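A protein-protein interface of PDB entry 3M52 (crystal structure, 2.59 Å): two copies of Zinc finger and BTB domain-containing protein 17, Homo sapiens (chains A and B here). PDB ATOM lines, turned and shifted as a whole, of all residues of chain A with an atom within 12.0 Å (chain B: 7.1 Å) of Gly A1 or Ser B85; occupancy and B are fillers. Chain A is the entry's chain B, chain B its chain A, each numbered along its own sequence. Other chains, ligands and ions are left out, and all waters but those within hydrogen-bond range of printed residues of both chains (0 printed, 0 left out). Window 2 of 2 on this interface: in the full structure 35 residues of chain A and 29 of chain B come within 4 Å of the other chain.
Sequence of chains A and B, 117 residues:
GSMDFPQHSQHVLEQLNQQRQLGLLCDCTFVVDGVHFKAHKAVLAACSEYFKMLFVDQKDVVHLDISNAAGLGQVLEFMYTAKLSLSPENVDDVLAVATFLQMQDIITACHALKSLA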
ATOM      1  N   GLY A   1      -5.435   4.097 -19.674  1.00  0.00           N
ATOM      2  CA  GLY A   1      -5.241   3.847 -18.215  1.00  0.00           C
ATOM      3  C   GLY A   1      -4.951   5.112 -17.429  1.00  0.00           C
ATOM      4  O   GLY A   1      -4.755   6.174 -18.015  1.00  0.00           O
ATOM      5  N   SER A   2      -4.918   4.994 -16.101  1.00  0.00           N
ATOM      6  CA  SER A   2      -4.834   6.157 -15.218  1.00  0.00           C
ATOM      7  C   SER A   2      -4.286   5.808 -13.825  1.00  0.00           C
ATOM      8  O   SER A   2      -4.806   4.912 -13.151  1.00  0.00           O
ATOM      9  CB  SER A   2      -6.216   6.821 -15.107  1.00  0.00           C
ATOM     10  OG  SER A   2      -6.236   7.854 -14.138  1.00  0.00           O
ATOM     11  N   MET A   3      -3.237   6.523 -13.411  1.00  0.00           N
ATOM     12  CA  MET A   3      -2.679   6.407 -12.058  1.00  0.00           C
ATOM     13  C   MET A   3      -2.870   7.706 -11.260  1.00  0.00           C
ATOM     14  O   MET A   3      -2.617   8.796 -11.771  1.00  0.00           O
ATOM     15  N   ASP A   4      -3.307   7.574 -10.009  1.00  0.00           N
ATOM     16  CA  ASP A   4      -3.581   8.721  -9.143  1.00  0.00           C
ATOM     17  C   ASP A   4      -2.331   9.165  -8.387  1.00  0.00           C
ATOM     18  O   ASP A   4      -1.663   8.352  -7.751  1.00  0.00           O
ATOM     19  N   PHE A   5      -2.016  10.457  -8.464  1.00  0.00           N
ATOM     20  CA  PHE A   5      -0.909  11.044  -7.699  1.00  0.00           C
ATOM     21  C   PHE A   5      -1.419  12.180  -6.796  1.00  0.00           C
ATOM     22  O   PHE A   5      -1.149  13.353  -7.082  1.00  0.00           O
ATOM     23  N   HIS A   8       0.008  15.668  -5.585  1.00  0.00           N
ATOM     24  CA  HIS A   8       0.082  16.786  -6.527  1.00  0.00           C
ATOM     25  C   HIS A   8      -0.900  17.924  -6.180  1.00  0.00           C
ATOM     26  O   HIS A   8      -0.620  19.084  -6.474  1.00  0.00           O
ATOM     27  CB  HIS A   8      -0.078  16.290  -7.968  1.00  0.00           C
ATOM     28  CG  HIS A   8      -0.309  17.381  -8.962  1.00  0.00           C
ATOM     29  ND1 HIS A   8       0.699  18.214  -9.405  1.00  0.00           N
ATOM     30  CD2 HIS A   8      -1.435  17.780  -9.600  1.00  0.00           C
ATOM     31  CE1 HIS A   8       0.201  19.076 -10.274  1.00  0.00           C
ATOM     32  NE2 HIS A   8      -1.091  18.835 -10.406  1.00  0.00           N
ATOM     33  N   GLN B  74      -1.113  14.816 -22.031  1.00  0.00           N
ATOM     34  CA  GLN B  74      -1.205  14.127 -20.749  1.00  0.00           C
ATOM     35  C   GLN B  74      -0.859  15.065 -19.588  1.00  0.00           C
ATOM     36  O   GLN B  74      -1.370  14.906 -18.481  1.00  0.00           O
ATOM     37  CB  GLN B  74      -0.280  12.907 -20.739  1.00  0.00           C
ATOM     38  CG  GLN B  74      -0.847  11.670 -21.447  1.00  0.00           C
ATOM     39  CD  GLN B  74      -0.765  11.725 -22.976  1.00  0.00           C
ATOM     40  OE1 GLN B  74      -1.580  11.118 -23.666  1.00  0.00           O
ATOM     41  NE2 GLN B  74       0.217  12.449 -23.506  1.00  0.00           N
ATOM     42  N   GLU B  77      -3.821  17.555 -18.451  1.00  0.00           N
ATOM     43  CA  GLU B  77      -4.809  16.788 -17.681  1.00  0.00           C
ATOM     44  C   GLU B  77      -4.332  16.521 -16.260  1.00  0.00           C
ATOM     45  O   GLU B  77      -5.105  16.668 -15.320  1.00  0.00           O
ATOM     46  CB  GLU B  77      -5.169  15.457 -18.363  1.00  0.00           C
ATOM     47  CG  GLU B  77      -6.425  15.478 -19.230  1.00  0.00           C
ATOM     48  CD  GLU B  77      -7.722  15.674 -18.438  1.00  0.00           C
ATOM     49  OE1 GLU B  77      -7.961  14.931 -17.455  1.00  0.00           O
ATOM     50  OE2 GLU B  77      -8.518  16.568 -18.816  1.00  0.00           O
ATOM     51  N   PHE B  78      -3.068  16.129 -16.115  1.00  0.00           N
ATOM     52  CA  PHE B  78      -2.484  15.848 -14.798  1.00  0.00           C
ATOM     53  C   PHE B  78      -2.589  17.055 -13.872  1.00  0.00           C
ATOM     54  O   PHE B  78      -3.021  16.923 -12.725  1.00  0.00           O
ATOM     55  CB  PHE B  78      -1.016  15.405 -14.914  1.00  0.00           C
ATOM     56  CG  PHE B  78      -0.377  15.044 -13.587  1.00  0.00           C
ATOM     57  CD1 PHE B  78       0.265  16.015 -12.813  1.00  0.00           C
ATOM     58  CD2 PHE B  78      -0.418  13.733 -13.112  1.00  0.00           C
ATOM     59  CE1 PHE B  78       0.854  15.687 -11.596  1.00  0.00           C
ATOM     60  CE2 PHE B  78       0.173  13.390 -11.886  1.00  0.00           C
ATOM     61  CZ  PHE B  78       0.814  14.373 -11.127  1.00  0.00           C
ATOM     62  N   LYS B  83      -4.126  12.900 -12.133  1.00  0.00           N
ATOM     63  CA  LYS B  83      -4.222  11.587 -12.760  1.00  0.00           C
ATOM     64  C   LYS B  83      -3.377  11.587 -14.028  1.00  0.00           C
ATOM     65  O   LYS B  83      -3.520  12.467 -14.886  1.00  0.00           O
ATOM     66  CB  LYS B  83      -5.673  11.264 -13.125  1.00  0.00           C
ATOM     67  CG  LYS B  83      -6.678  11.408 -11.991  1.00  0.00           C
ATOM     68  CD  LYS B  83      -6.949  10.085 -11.290  1.00  0.00           C
ATOM     69  CE  LYS B  83      -8.340  10.070 -10.671  1.00  0.00           C
ATOM     70  NZ  LYS B  83      -8.455  11.070  -9.574  1.00  0.00           N
ATOM     71  N   LEU B  84      -2.500  10.597 -14.145  1.00  0.00           N
ATOM     72  CA  LEU B  84      -1.600  10.498 -15.295  1.00  0.00           C
ATOM     73  C   LEU B  84      -1.968   9.308 -16.190  1.00  0.00           C
ATOM     74  O   LEU B  84      -2.194   8.202 -15.695  1.00  0.00           O
ATOM     75  CB  LEU B  84      -0.137  10.416 -14.821  1.00  0.00           C
ATOM     76  CG  LEU B  84       0.981  10.802 -15.801  1.00  0.00           C
ATOM     77  CD1 LEU B  84       0.810  12.237 -16.330  1.00  0.00           C
ATOM     78  CD2 LEU B  84       2.342  10.611 -15.152  1.00  0.00           C
ATOM     79  N   SER B  85      -2.040   9.548 -17.500  1.00  0.00           N
ATOM     80  CA  SER B  85      -2.414   8.497 -18.454  1.00  0.00           C
ATOM     81  C   SER B  85      -1.209   7.971 -19.212  1.00  0.00           C
ATOM     82  O   SER B  85      -0.918   8.405 -20.333  1.00  0.00           O
ATOM     83  CB  SER B  85      -3.495   8.983 -19.417  1.00  0.00           C
ATOM     84  OG  SER B  85      -4.728   9.137 -18.738  1.00  0.00           O
ATOM     85  N   LEU B  86      -0.512   7.033 -18.580  1.00  0.00           N
ATOM     86  CA  LEU B  86       0.691   6.435 -19.140  1.00  0.00           C
ATOM     87  C   LEU B  86       0.394   5.127 -19.861  1.00  0.00           C
ATOM     88  O   LEU B  86      -0.549   4.405 -19.517  1.00  0.00           O
ATOM     89  CB  LEU B  86       1.727   6.186 -18.039  1.00  0.00           C
ATOM     90  CG  LEU B  86       2.238   7.363 -17.198  1.00  0.00           C
ATOM     91  CD1 LEU B  86       2.934   6.856 -15.933  1.00  0.00           C
ATOM     92  CD2 LEU B  86       3.161   8.285 -18.001  1.00  0.00           C
ATOM     93  N   SER B  87       1.221   4.832 -20.857  1.00  0.00           N
ATOM     94  CA  SER B  87       1.191   3.573 -21.582  1.00  0.00           C
ATOM     95  C   SER B  87       2.629   3.242 -21.979  1.00  0.00           C
ATOM     96  O   SER B  87       3.472   4.141 -22.037  1.00  0.00           O
ATOM     97  CB  SER B  87       0.307   3.698 -22.817  1.00  0.00           C
ATOM     98  OG  SER B  87       0.706   4.805 -23.603  1.00  0.00           O
ATOM     99  N   ASN B  90       3.952   5.768 -24.350  1.00  0.00           N
ATOM    100  CA  ASN B  90       4.100   7.194 -24.005  1.00  0.00           C
ATOM    101  C   ASN B  90       4.896   7.605 -22.742  1.00  0.00           C
ATOM    102  O   ASN B  90       5.076   8.801 -22.509  1.00  0.00           O
ATOM    103  CB  ASN B  90       2.747   7.935 -24.118  1.00  0.00           C
ATOM    104  CG  ASN B  90       1.892   7.819 -22.868  1.00  0.00           C
ATOM    105  OD1 ASN B  90       2.159   7.010 -21.980  1.00  0.00           O
ATOM    106  ND2 ASN B  90       0.854   8.647 -22.790  1.00  0.00           N
ATOM    107  N   VAL B  91       5.394   6.647 -21.955  1.00  0.00           N
ATOM    108  CA  VAL B  91       6.110   6.974 -20.695  1.00  0.00           C
ATOM    109  C   VAL B  91       7.323   7.903 -20.855  1.00  0.00           C
ATOM    110  O   VAL B  91       7.493   8.853 -20.078  1.00  0.00           O
ATOM    111  CB  VAL B  91       6.611   5.726 -19.914  1.00  0.00           C
ATOM    112  CG1 VAL B  91       6.835   6.089 -18.446  1.00  0.00           C
ATOM    113  CG2 VAL B  91       5.633   4.597 -20.003  1.00  0.00           C
ATOM    114  N   VAL B  94       6.286  11.574 -22.021  1.00  0.00           N
ATOM    115  CA  VAL B  94       5.735  12.301 -20.873  1.00  0.00           C
ATOM    116  C   VAL B  94       6.854  12.694 -19.895  1.00  0.00           C
ATOM    117  O   VAL B  94       6.889  13.826 -19.407  1.00  0.00           O
ATOM    118  CB  VAL B  94       4.603  11.501 -20.142  1.00  0.00           C
ATOM    119  CG1 VAL B  94       4.208  12.171 -18.821  1.00  0.00           C
ATOM    120  CG2 VAL B  94       3.373  11.335 -21.036  1.00  0.00           C
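N of Leu B84 sits at hydrogen-bond distance from O of Met A3 (3.0 Å).
The side-chain hydroxyl (OG) of Ser B85 is in hydrogen-bond range of the backbone carbonyl oxygen (O) of Gly A1 (3.1 Å).
The backbone carbonyl oxygen (O) of Ser B85 sits at hydrogen-bond distance from the side-chain amide nitrogen (ND2) of Asn B90.
Among the printed residues, merely in contact across the chains: Ser A2 with Lys B83 (3.6 Å), Ser A2 with Leu B84 (3.4 Å), Met A3 with Lys B83 (3.4 Å) and His A8 with Phe B78 (3.3 Å).
Of the printed residues of chain B, Gly A1 touches Ser B85.
Printed residues of chain B within 4 Å of Met A3: Lys B83 (3.4 Å) and Leu B84 (3.0 Å).
Printed residues of chain B within 4 Å of His A8: Phe B78 (3.3 Å).
No residue of chain A comes within 4 Å of Gln B74.
Of chain A, only Gly A1 comes within 4 Å of Ser B85.
No residue of chain A comes within 4 Å of Asn B90.
Val B91 touches none of the printed residues of chain A.
The nearest residue of chain A that does not touch Ser B85 is Ser A2 (4.6 Å).
The nearest printed residue of chain B that does not touch Ser A2 is Ser B85 (4.6 Å).
Printed residues of chain A that touch a printed residue of chain B: Gly A1, Ser A2, Met A3 and His A8.
Hydrophobic or aromatic side chains of chain A within 4 Å of the printed part of chain B: His A8.
No position is printed for both chains.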
